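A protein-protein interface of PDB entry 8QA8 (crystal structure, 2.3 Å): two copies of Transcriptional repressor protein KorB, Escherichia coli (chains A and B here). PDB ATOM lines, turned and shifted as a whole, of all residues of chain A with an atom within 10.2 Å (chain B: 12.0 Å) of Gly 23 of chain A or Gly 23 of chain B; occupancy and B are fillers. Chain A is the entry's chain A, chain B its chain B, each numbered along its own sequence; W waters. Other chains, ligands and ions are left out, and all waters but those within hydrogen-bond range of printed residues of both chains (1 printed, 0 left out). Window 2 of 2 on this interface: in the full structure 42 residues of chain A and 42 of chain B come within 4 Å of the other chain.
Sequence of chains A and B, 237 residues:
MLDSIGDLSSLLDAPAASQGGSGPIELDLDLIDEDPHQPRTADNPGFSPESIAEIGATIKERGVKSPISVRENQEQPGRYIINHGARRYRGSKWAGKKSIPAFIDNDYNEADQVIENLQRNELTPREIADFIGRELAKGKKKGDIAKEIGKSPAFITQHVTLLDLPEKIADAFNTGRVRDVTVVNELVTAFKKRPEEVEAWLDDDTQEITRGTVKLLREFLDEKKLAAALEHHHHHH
Water W1 lies within hydrogen-bond range of OD2 of Asp 105 of chain A (2.6 Å) and O of Lys 65 of chain B (2.9 Å).
The backbone NH of Val 70 of chain B is in hydrogen-bond range of the backbone carbonyl oxygen of Phe 103 of chain B, at 2.9 Å. The backbone carbonyl oxygen (O) of Val 70 of chain A sits at hydrogen-bond distance from the backbone NH (N) of Asp 105 of chain A. O of Phe 103 of chain A lies within hydrogen-bond range of N of Val 70 of chain A (3.0 Å). The backbone carbonyl oxygen of Ile 68 of chain A is in hydrogen-bond range of the backbone NH of Phe 103 of chain A (2.9 Å). The backbone carbonyl oxygen of Ile 68 of chain B is in hydrogen-bond range of the backbone NH of Phe 103 of chain B, 2.9 Å away.
Among the printed residues, merely in contact across the chains: Pro 67 of chain A with Phe 103 of chain B, Phe 103 of chain A with Lys 65 of chain B and Phe 103 of chain A with Pro 67 of chain B.
Gly 23 of chain A touches its own counterpart, Gly 23 of chain B. Pro 67 of chain A touches Phe 103 of chain B, and with the chains exchanged Phe 103 of chain A touches Pro 67 of chain B.
Printed residues of chain A within 4 Å of Gly 23 of chain B: Gly 23 (3.0 Å). No residue of chain B comes within 4 Å of Ile 25 of chain A. Printed residues of chain B within 4 Å of Asp 105 of chain A: Lys 65. Of the printed residues of chain A, Lys 65 of chain B touches Phe 103 (3.1 Å) and Asp 105 (2.9 Å). Printed residues of chain B within 4 Å of Phe 103 of chain A: Lys 65 (3.1 Å) and Pro 67 (3.2 Å). The nearest printed residue of chain B that does not touch Gly 23 of chain A is Pro 24 of chain B (4.7 Å). The nearest printed residue of chain B that does not touch Asp 105 of chain A is Val 64 of chain B (6.1 Å).
Of the 14 printed residues of chain A, 4 touch a printed residue of chain B. Printed residues of chain A that touch a printed residue of chain B: Gly 23, Pro 67, Phe 103 and Asp 105. Of the 21 printed residues of chain B, 4 touch a printed residue of chain A. Hydrophobic or aromatic side chains of chain B that line the printed part of chain A: Pro 67 and Phe 103. Among the printed residues, 5 pairs touch across the chains. Among the printed residues, Asp or Glu carboxylates within 4 Å of a Lys or Arg side-chain nitrogen of the other chain: Asp 105 of chain A with Lys 65 of chain B (2.9 Å).
N of Gly 23 of chain A sits at hydrogen-bond distance from O of Gly 23 of chain B (3.3 Å). The side-chain amino group of Lys 65 of chain B lies within salt-bridge range of the side-chain carboxylate of Asp 105 of chain A, at 2.9 Å.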
ATOM      1  N   GLY A  23      12.908 -18.705  13.804  1.00  0.00           N
ATOM      2  CA  GLY A  23      13.939 -17.918  14.526  1.00  0.00           C
ATOM      3  C   GLY A  23      13.415 -16.637  15.210  1.00  0.00           C
ATOM      4  O   GLY A  23      12.353 -16.120  14.836  1.00  0.00           O
ATOM      5  N   PRO A  24      14.165 -16.055  16.192  1.00  0.00           N
ATOM      6  CA  PRO A  24      13.916 -14.710  16.706  1.00  0.00           C
ATOM      7  C   PRO A  24      14.421 -13.664  15.714  1.00  0.00           C
ATOM      8  O   PRO A  24      15.263 -13.952  14.876  1.00  0.00           O
ATOM      9  CB  PRO A  24      14.715 -14.605  18.018  1.00  0.00           C
ATOM     10  CG  PRO A  24      15.855 -15.575  17.825  1.00  0.00           C
ATOM     11  CD  PRO A  24      15.374 -16.621  16.818  1.00  0.00           C
ATOM     12  N   ILE A  25      13.844 -12.467  15.772  1.00  0.00           N
ATOM     13  CA  ILE A  25      14.199 -11.409  14.848  1.00  0.00           C
ATOM     14  C   ILE A  25      15.190 -10.497  15.569  1.00  0.00           C
ATOM     15  O   ILE A  25      15.118 -10.328  16.777  1.00  0.00           O
ATOM     16  CB  ILE A  25      12.928 -10.734  14.288  1.00  0.00           C
ATOM     17  CG1 ILE A  25      13.221  -9.874  13.054  1.00  0.00           C
ATOM     18  CG2 ILE A  25      12.159  -9.992  15.354  1.00  0.00           C
ATOM     19  CD1 ILE A  25      13.613 -10.663  11.784  1.00  0.00           C
ATOM     20  N   GLU A  26      16.210 -10.030  14.846  1.00  0.00           N
ATOM     21  CA  GLU A  26      17.132  -9.040  15.398  1.00  0.00           C
ATOM     22  C   GLU A  26      16.493  -7.665  15.176  1.00  0.00           C
ATOM     23  O   GLU A  26      16.352  -7.203  14.045  1.00  0.00           O
ATOM     24  CB  GLU A  26      18.544  -9.169  14.800  1.00  0.00           C
ATOM     25  CG  GLU A  26      19.361 -10.337  15.374  1.00  0.00           C
ATOM     26  CD  GLU A  26      19.989 -10.187  16.757  1.00  0.00           C
ATOM     27  OE1 GLU A  26      20.002  -9.050  17.317  1.00  0.00           O
ATOM     28  OE2 GLU A  26      20.460 -11.245  17.305  1.00  0.00           O
ATOM     29  N   LEU A  27      16.050  -7.031  16.257  1.00  0.00           N
ATOM     30  CA  LEU A  27      15.303  -5.789  16.135  1.00  0.00           C
ATOM     31  C   LEU A  27      16.179  -4.615  16.525  1.00  0.00           C
ATOM     32  O   LEU A  27      16.729  -4.617  17.631  1.00  0.00           O
ATOM     33  CB  LEU A  27      14.088  -5.819  17.059  1.00  0.00           C
ATOM     34  CG  LEU A  27      12.777  -6.343  16.479  1.00  0.00           C
ATOM     35  CD1 LEU A  27      11.597  -5.850  17.321  1.00  0.00           C
ATOM     36  CD2 LEU A  27      12.623  -5.999  15.015  1.00  0.00           C
ATOM     37  N   PRO A  67      15.369 -14.139  24.007  1.00  0.00           N
ATOM     38  CA  PRO A  67      14.857 -13.021  23.227  1.00  0.00           C
ATOM     39  C   PRO A  67      13.706 -12.313  23.945  1.00  0.00           C
ATOM     40  O   PRO A  67      12.930 -12.935  24.632  1.00  0.00           O
ATOM     41  CB  PRO A  67      14.367 -13.677  21.935  1.00  0.00           C
ATOM     42  CG  PRO A  67      15.161 -14.979  21.830  1.00  0.00           C
ATOM     43  CD  PRO A  67      15.365 -15.421  23.281  1.00  0.00           C
ATOM     44  N   ILE A  68      13.619 -10.979  23.802  1.00  0.00           N
ATOM     45  CA  ILE A  68      12.564 -10.229  24.466  1.00  0.00           C
ATOM     46  C   ILE A  68      11.263 -10.413  23.698  1.00  0.00           C
ATOM     47  O   ILE A  68      11.270 -10.839  22.539  1.00  0.00           O
ATOM     48  CB  ILE A  68      12.931  -8.745  24.632  1.00  0.00           C
ATOM     49  CG1 ILE A  68      13.098  -8.013  23.298  1.00  0.00           C
ATOM     50  CG2 ILE A  68      14.165  -8.602  25.489  1.00  0.00           C
ATOM     51  CD1 ILE A  68      13.003  -6.495  23.447  1.00  0.00           C
ATOM     52  N   VAL A  70       7.953  -8.341  22.274  1.00  0.00           N
ATOM     53  CA  VAL A  70       7.439  -7.025  21.975  1.00  0.00           C
ATOM     54  C   VAL A  70       6.089  -7.153  21.281  1.00  0.00           C
ATOM     55  O   VAL A  70       5.773  -8.174  20.665  1.00  0.00           O
ATOM     56  CB  VAL A  70       8.426  -6.232  21.094  1.00  0.00           C
ATOM     57  CG1 VAL A  70       9.782  -6.061  21.756  1.00  0.00           C
ATOM     58  CG2 VAL A  70       8.584  -6.872  19.723  1.00  0.00           C
ATOM     59  N   ILE A 100      18.536  -6.256  19.201  1.00  0.00           N
ATOM     60  CA  ILE A 100      18.233  -7.209  20.248  1.00  0.00           C
ATOM     61  C   ILE A 100      17.351  -8.300  19.667  1.00  0.00           C
ATOM     62  O   ILE A 100      16.461  -8.025  18.858  1.00  0.00           O
ATOM     63  CB  ILE A 100      17.565  -6.513  21.454  1.00  0.00           C
ATOM     64  CG1 ILE A 100      17.466  -7.435  22.663  1.00  0.00           C
ATOM     65  CG2 ILE A 100      16.206  -5.950  21.077  1.00  0.00           C
ATOM     66  CD1 ILE A 100      17.095  -6.728  23.938  1.00  0.00           C
ATOM     67  N   PRO A 101      17.597  -9.569  20.046  1.00  0.00           N
ATOM     68  CA  PRO A 101      16.758 -10.682  19.624  1.00  0.00           C
ATOM     69  C   PRO A 101      15.366 -10.531  20.231  1.00  0.00           C
ATOM     70  O   PRO A 101      15.218 -10.295  21.431  1.00  0.00           O
ATOM     71  CB  PRO A 101      17.463 -11.939  20.199  1.00  0.00           C
ATOM     72  CG  PRO A 101      18.845 -11.497  20.602  1.00  0.00           C
ATOM     73  CD  PRO A 101      18.717 -10.020  20.893  1.00  0.00           C
ATOM     74  N   ALA A 102      14.343 -10.738  19.410  1.00  0.00           N
ATOM     75  CA  ALA A 102      12.996 -10.530  19.896  1.00  0.00           C
ATOM     76  C   ALA A 102      11.990 -11.376  19.138  1.00  0.00           C
ATOM     77  O   ALA A 102      12.272 -11.816  18.030  1.00  0.00           O
ATOM     78  CB  ALA A 102      12.626  -9.051  19.765  1.00  0.00           C
ATOM     79  N   PHE A 103      10.820 -11.584  19.754  1.00  0.00           N
ATOM     80  CA  PHE A 103       9.673 -12.114  19.039  1.00  0.00           C
ATOM     81  C   PHE A 103       8.506 -11.154  19.248  1.00  0.00           C
ATOM     82  O   PHE A 103       8.441 -10.444  20.250  1.00  0.00           O
ATOM     83  CB  PHE A 103       9.304 -13.541  19.478  1.00  0.00           C
ATOM     84  CG  PHE A 103       9.063 -13.747  20.951  1.00  0.00           C
ATOM     85  CD1 PHE A 103       7.794 -14.043  21.424  1.00  0.00           C
ATOM     86  CD2 PHE A 103      10.110 -13.680  21.861  1.00  0.00           C
ATOM     87  CE1 PHE A 103       7.573 -14.229  22.776  1.00  0.00           C
ATOM     88  CE2 PHE A 103       9.887 -13.860  23.219  1.00  0.00           C
ATOM     89  CZ  PHE A 103       8.615 -14.120  23.676  1.00  0.00           C
ATOM     90  N   ILE A 104       7.586 -11.181  18.286  1.00  0.00           N
ATOM     91  CA  ILE A 104       6.393 -10.390  18.337  1.00  0.00           C
ATOM     92  C   ILE A 104       5.257 -11.230  18.939  1.00  0.00           C
ATOM     93  O   ILE A 104       4.940 -12.298  18.450  1.00  0.00           O
ATOM     94  CB  ILE A 104       6.070  -9.888  16.925  1.00  0.00           C
ATOM     95  CG1 ILE A 104       7.168  -8.958  16.420  1.00  0.00           C
ATOM     96  CG2 ILE A 104       4.727  -9.192  16.910  1.00  0.00           C
ATOM     97  CD1 ILE A 104       7.069  -8.622  14.952  1.00  0.00           C
ATOM     98  N   ASP A 105       4.630 -10.687  19.988  1.00  0.00           N
ATOM     99  CA  ASP A 105       3.457 -11.262  20.610  1.00  0.00           C
ATOM    100  C   ASP A 105       2.458 -10.132  20.897  1.00  0.00           C
ATOM    101  O   ASP A 105       2.621  -9.354  21.843  1.00  0.00           O
ATOM    102  CB  ASP A 105       3.874 -11.973  21.889  1.00  0.00           C
ATOM    103  CG  ASP A 105       2.763 -12.698  22.616  1.00  0.00           C
ATOM    104  OD1 ASP A 105       1.620 -12.653  22.123  1.00  0.00           O
ATOM    105  OD2 ASP A 105       3.088 -13.349  23.655  1.00  0.00           O
ATOM    106  N   GLY B  23       8.673 -16.170  13.922  1.00  0.00           N
ATOM    107  CA  GLY B  23       8.497 -16.210  15.398  1.00  0.00           C
ATOM    108  C   GLY B  23       9.187 -17.400  16.085  1.00  0.00           C
ATOM    109  O   GLY B  23      10.142 -17.958  15.535  1.00  0.00           O
ATOM    110  N   PRO B  24       8.724 -17.833  17.295  1.00  0.00           N
ATOM    111  CA  PRO B  24       9.166 -19.078  17.930  1.00  0.00           C
ATOM    112  C   PRO B  24       8.493 -20.263  17.258  1.00  0.00           C
ATOM    113  O   PRO B  24       7.457 -20.111  16.597  1.00  0.00           O
ATOM    114  CB  PRO B  24       8.676 -18.996  19.382  1.00  0.00           C
ATOM    115  CG  PRO B  24       7.448 -18.080  19.322  1.00  0.00           C
ATOM    116  CD  PRO B  24       7.683 -17.181  18.113  1.00  0.00           C
ATOM    117  N   ILE B  25       9.118 -21.438  17.385  1.00  0.00           N
ATOM    118  CA  ILE B  25       8.569 -22.642  16.791  1.00  0.00           C
ATOM    119  C   ILE B  25       7.758 -23.335  17.879  1.00  0.00           C
ATOM    120  O   ILE B  25       8.162 -23.298  19.046  1.00  0.00           O
ATOM    121  CB  ILE B  25       9.724 -23.514  16.282  1.00  0.00           C
ATOM    122  CG1 ILE B  25      10.729 -22.736  15.420  1.00  0.00           C
ATOM    123  CG2 ILE B  25       9.198 -24.754  15.577  1.00  0.00           C
ATOM    124  CD1 ILE B  25      12.171 -22.947  15.852  1.00  0.00           C
ATOM    125  N   GLU B  26       6.590 -23.902  17.505  1.00  0.00           N
ATOM    126  CA  GLU B  26       5.882 -24.764  18.430  1.00  0.00           C
ATOM    127  C   GLU B  26       6.498 -26.160  18.309  1.00  0.00           C
ATOM    128  O   GLU B  26       6.336 -26.836  17.300  1.00  0.00           O
ATOM    129  CB  GLU B  26       4.380 -24.731  18.148  1.00  0.00           C
ATOM    130  CG  GLU B  26       3.624 -23.505  18.691  1.00  0.00           C
ATOM    131  CD  GLU B  26       3.429 -23.364  20.207  1.00  0.00           C
ATOM    132  OE1 GLU B  26       3.614 -24.363  20.952  1.00  0.00           O
ATOM    133  OE2 GLU B  26       3.082 -22.252  20.647  1.00  0.00           O
ATOM    134  N   LEU B  27       7.277 -26.577  19.319  1.00  0.00           N
ATOM    135  CA  LEU B  27       8.040 -27.803  19.242  1.00  0.00           C
ATOM    136  C   LEU B  27       7.311 -28.887  20.029  1.00  0.00           C
ATOM    137  O   LEU B  27       7.032 -28.696  21.207  1.00  0.00           O
ATOM    138  CB  LEU B  27       9.421 -27.532  19.847  1.00  0.00           C
ATOM    139  CG  LEU B  27      10.559 -28.441  19.381  1.00  0.00           C
ATOM    140  CD1 LEU B  27      10.618 -28.562  17.864  1.00  0.00           C
ATOM    141  CD2 LEU B  27      11.888 -27.974  19.940  1.00  0.00           C
ATOM    142  N   VAL B  64       3.151 -20.600  27.501  1.00  0.00           N
ATOM    143  CA  VAL B  64       4.503 -20.190  27.800  1.00  0.00           C
ATOM    144  C   VAL B  64       4.740 -18.874  27.075  1.00  0.00           C
ATOM    145  O   VAL B  64       4.590 -18.790  25.847  1.00  0.00           O
ATOM    146  CB  VAL B  64       5.502 -21.246  27.339  1.00  0.00           C
ATOM    147  CG1 VAL B  64       6.932 -20.702  27.397  1.00  0.00           C
ATOM    148  CG2 VAL B  64       5.368 -22.537  28.140  1.00  0.00           C
ATOM    149  N   LYS B  65       5.078 -17.838  27.846  1.00  0.00           N
ATOM    150  CA  LYS B  65       5.215 -16.505  27.251  1.00  0.00           C
ATOM    151  C   LYS B  65       6.668 -16.214  26.863  1.00  0.00           C
ATOM    152  O   LYS B  65       6.892 -15.385  25.981  1.00  0.00           O
ATOM    153  CB  LYS B  65       4.602 -15.428  28.160  1.00  0.00           C
ATOM    154  CG  LYS B  65       3.075 -15.353  28.108  1.00  0.00           C
ATOM    155  CD  LYS B  65       2.595 -15.143  26.686  1.00  0.00           C
ATOM    156  CE  LYS B  65       1.204 -14.541  26.559  1.00  0.00           C
ATOM    157  NZ  LYS B  65       0.849 -14.486  25.120  1.00  0.00           N
ATOM    158  N   SER B  66       7.636 -16.900  27.499  1.00  0.00           N
ATOM    159  CA  SER B  66       9.052 -16.804  27.140  1.00  0.00           C
ATOM    160  C   SER B  66       9.534 -18.127  26.546  1.00  0.00           C
ATOM    161  O   SER B  66       9.815 -19.080  27.266  1.00  0.00           O
ATOM    162  CB  SER B  66       9.895 -16.448  28.331  1.00  0.00           C
ATOM    163  OG  SER B  66       9.463 -15.233  28.909  1.00  0.00           O
ATOM    164  N   PRO B  67       9.654 -18.234  25.216  1.00  0.00           N
ATOM    165  CA  PRO B  67       9.994 -19.498  24.586  1.00  0.00           C
ATOM    166  C   PRO B  67      11.268 -20.095  25.174  1.00  0.00           C
ATOM    167  O   PRO B  67      12.186 -19.363  25.547  1.00  0.00           O
ATOM    168  CB  PRO B  67      10.181 -19.123  23.115  1.00  0.00           C
ATOM    169  CG  PRO B  67       9.349 -17.884  22.926  1.00  0.00           C
ATOM    170  CD  PRO B  67       9.459 -17.149  24.246  1.00  0.00           C
ATOM    171  N   ILE B  68      11.314 -21.426  25.258  1.00  0.00           N
ATOM    172  CA  ILE B  68      12.507 -22.072  25.779  1.00  0.00           C
ATOM    173  C   ILE B  68      13.591 -22.067  24.704  1.00  0.00           C
ATOM    174  O   ILE B  68      13.296 -21.860  23.527  1.00  0.00           O
ATOM    175  CB  ILE B  68      12.215 -23.512  26.278  1.00  0.00           C
ATOM    176  CG1 ILE B  68      11.758 -24.458  25.178  1.00  0.00           C
ATOM    177  CG2 ILE B  68      11.206 -23.465  27.398  1.00  0.00           C
ATOM    178  CD1 ILE B  68      11.891 -25.928  25.570  1.00  0.00           C
ATOM    179  N   SER B  69      14.832 -22.301  25.137  1.00  0.00           N
ATOM    180  CA  SER B  69      15.964 -22.426  24.234  1.00  0.00           C
ATOM    181  C   SER B  69      16.399 -23.886  24.196  1.00  0.00           C
ATOM    182  O   SER B  69      16.655 -24.447  25.242  1.00  0.00           O
ATOM    183  CB  SER B  69      17.108 -21.540  24.670  1.00  0.00           C
ATOM    184  OG  SER B  69      18.233 -21.641  23.809  1.00  0.00           O
ATOM    185  N   VAL B  70      16.531 -24.451  22.995  1.00  0.00           N
ATOM    186  CA  VAL B  70      17.016 -25.819  22.849  1.00  0.00           C
ATOM    187  C   VAL B  70      18.178 -25.864  21.858  1.00  0.00           C
ATOM    188  O   VAL B  70      18.312 -24.996  21.007  1.00  0.00           O
ATOM    189  CB  VAL B  70      15.880 -26.757  22.397  1.00  0.00           C
ATOM    190  CG1 VAL B  70      14.724 -26.768  23.390  1.00  0.00           C
ATOM    191  CG2 VAL B  70      15.395 -26.411  21.000  1.00  0.00           C
ATOM    192  N   GLU B  72      20.111 -28.766  19.070  1.00  0.00           N
ATOM    193  CA  GLU B  72      19.971 -30.010  18.346  1.00  0.00           C
ATOM    194  C   GLU B  72      20.805 -31.066  19.049  1.00  0.00           C
ATOM    195  O   GLU B  72      21.954 -30.823  19.362  1.00  0.00           O
ATOM    196  CB  GLU B  72      20.359 -29.820  16.874  1.00  0.00           C
ATOM    197  CG  GLU B  72      19.357 -28.930  16.178  1.00  0.00           C
ATOM    198  CD  GLU B  72      19.607 -28.423  14.790  1.00  0.00           C
ATOM    199  OE1 GLU B  72      20.761 -28.044  14.476  1.00  0.00           O
ATOM    200  OE2 GLU B  72      18.609 -28.248  14.117  1.00  0.00           O
ATOM    201  N   TYR B  80      16.014 -32.737  20.484  1.00  0.00           N
ATOM    202  CA  TYR B  80      16.562 -31.501  21.012  1.00  0.00           C
ATOM    203  C   TYR B  80      16.862 -31.663  22.498  1.00  0.00           C
ATOM    204  O   TYR B  80      16.184 -32.414  23.193  1.00  0.00           O
ATOM    205  CB  TYR B  80      15.571 -30.349  20.780  1.00  0.00           C
ATOM    206  CG  TYR B  80      15.196 -30.156  19.334  1.00  0.00           C
ATOM    207  CD1 TYR B  80      15.926 -29.353  18.500  1.00  0.00           C
ATOM    208  CD2 TYR B  80      14.122 -30.814  18.791  1.00  0.00           C
ATOM    209  CE1 TYR B  80      15.620 -29.237  17.155  1.00  0.00           C
ATOM    210  CE2 TYR B  80      13.783 -30.688  17.454  1.00  0.00           C
ATOM    211  CZ  TYR B  80      14.552 -29.913  16.620  1.00  0.00           C
ATOM    212  OH  TYR B  80      14.299 -29.763  15.269  1.00  0.00           O
ATOM    213  N   ILE B 100       5.566 -26.821  22.873  1.00  0.00           N
ATOM    214  CA  ILE B 100       6.075 -25.708  23.652  1.00  0.00           C
ATOM    215  C   ILE B 100       6.780 -24.746  22.703  1.00  0.00           C
ATOM    216  O   ILE B 100       7.448 -25.158  21.757  1.00  0.00           O
ATOM    217  CB  ILE B 100       7.012 -26.181  24.772  1.00  0.00           C
ATOM    218  CG1 ILE B 100       7.401 -25.043  25.714  1.00  0.00           C
ATOM    219  CG2 ILE B 100       8.252 -26.858  24.197  1.00  0.00           C
ATOM    220  CD1 ILE B 100       8.042 -25.520  26.979  1.00  0.00           C
ATOM    221  N   PRO B 101       6.595 -23.424  22.888  1.00  0.00           N
ATOM    222  CA  PRO B 101       7.285 -22.418  22.085  1.00  0.00           C
ATOM    223  C   PRO B 101       8.778 -22.479  22.346  1.00  0.00           C
ATOM    224  O   PRO B 101       9.203 -22.480  23.503  1.00  0.00           O
ATOM    225  CB  PRO B 101       6.726 -21.065  22.571  1.00  0.00           C
ATOM    226  CG  PRO B 101       5.434 -21.414  23.292  1.00  0.00           C
ATOM    227  CD  PRO B 101       5.667 -22.810  23.854  1.00  0.00           C
ATOM    228  N   ALA B 102       9.578 -22.505  21.272  1.00  0.00           N
ATOM    229  CA  ALA B 102      11.008 -22.644  21.461  1.00  0.00           C
ATOM    230  C   ALA B 102      11.784 -21.977  20.335  1.00  0.00           C
ATOM    231  O   ALA B 102      11.243 -21.743  19.241  1.00  0.00           O
ATOM    232  CB  ALA B 102      11.354 -24.108  21.520  1.00  0.00           C
ATOM    233  N   PHE B 103      13.055 -21.664  20.630  1.00  0.00           N
ATOM    234  CA  PHE B 103      14.014 -21.321  19.593  1.00  0.00           C
ATOM    235  C   PHE B 103      15.214 -22.250  19.711  1.00  0.00           C
ATOM    236  O   PHE B 103      15.506 -22.804  20.777  1.00  0.00           O
ATOM    237  CB  PHE B 103      14.435 -19.843  19.645  1.00  0.00           C
ATOM    238  CG  PHE B 103      15.021 -19.364  20.947  1.00  0.00           C
ATOM    239  CD1 PHE B 103      16.358 -19.014  21.025  1.00  0.00           C
ATOM    240  CD2 PHE B 103      14.222 -19.247  22.067  1.00  0.00           C
ATOM    241  CE1 PHE B 103      16.889 -18.548  22.210  1.00  0.00           C
ATOM    242  CE2 PHE B 103      14.757 -18.805  23.263  1.00  0.00           C
ATOM    243  CZ  PHE B 103      16.095 -18.462  23.325  1.00  0.00           C
ATOM    244  N   ILE B 104      15.910 -22.415  18.581  1.00  0.00           N
ATOM    245  CA  ILE B 104      17.103 -23.227  18.528  1.00  0.00           C
ATOM    246  C   ILE B 104      18.316 -22.321  18.689  1.00  0.00           C
ATOM    247  O   ILE B 104      18.476 -21.372  17.941  1.00  0.00           O
ATOM    248  CB  ILE B 104      17.129 -24.013  17.207  1.00  0.00           C
ATOM    249  CG1 ILE B 104      15.942 -24.972  17.127  1.00  0.00           C
ATOM    250  CG2 ILE B 104      18.465 -24.724  17.024  1.00  0.00           C
ATOM    251  CD1 ILE B 104      15.773 -25.568  15.746  1.00  0.00           C
ATOM    252  N   ASP B 105      19.171 -22.640  19.661  1.00  0.00           N
ATOM    253  CA  ASP B 105      20.474 -22.010  19.819  1.00  0.00           C
ATOM    254  C   ASP B 105      21.536 -23.089  20.054  1.00  0.00           C
ATOM    255  O   ASP B 105      21.612 -23.660  21.139  1.00  0.00           O
ATOM    256  CB  ASP B 105      20.392 -21.022  20.987  1.00  0.00           C
ATOM    257  CG  ASP B 105      21.654 -20.229  21.259  1.00  0.00           C
ATOM    258  OD1 ASP B 105      22.670 -20.436  20.550  1.00  0.00           O
ATOM    259  OD2 ASP B 105      21.613 -19.413  22.184  1.00  0.00           O
ATOM    260  N   ASN B 106      22.361 -23.341  19.039  1.00  0.00           N
ATOM    261  CA  ASN B 106      23.397 -24.366  19.134  1.00  0.00           C
ATOM    262  C   ASN B 106      24.691 -23.820  19.721  1.00  0.00           C
ATOM    263  O   ASN B 106      25.637 -24.568  19.881  1.00  0.00           O
ATOM    264  CB  ASN B 106      23.663 -25.032  17.784  1.00  0.00           C
ATOM    265  CG  ASN B 106      22.506 -25.908  17.361  1.00  0.00           C
ATOM    266  OD1 ASN B 106      21.915 -26.612  18.177  1.00  0.00           O
ATOM    267  ND2 ASN B 106      22.143 -25.824  16.096  1.00  0.00           N
HETATM  268  O   HOH W   1       5.533 -13.220  24.642  1.00  0.00           O
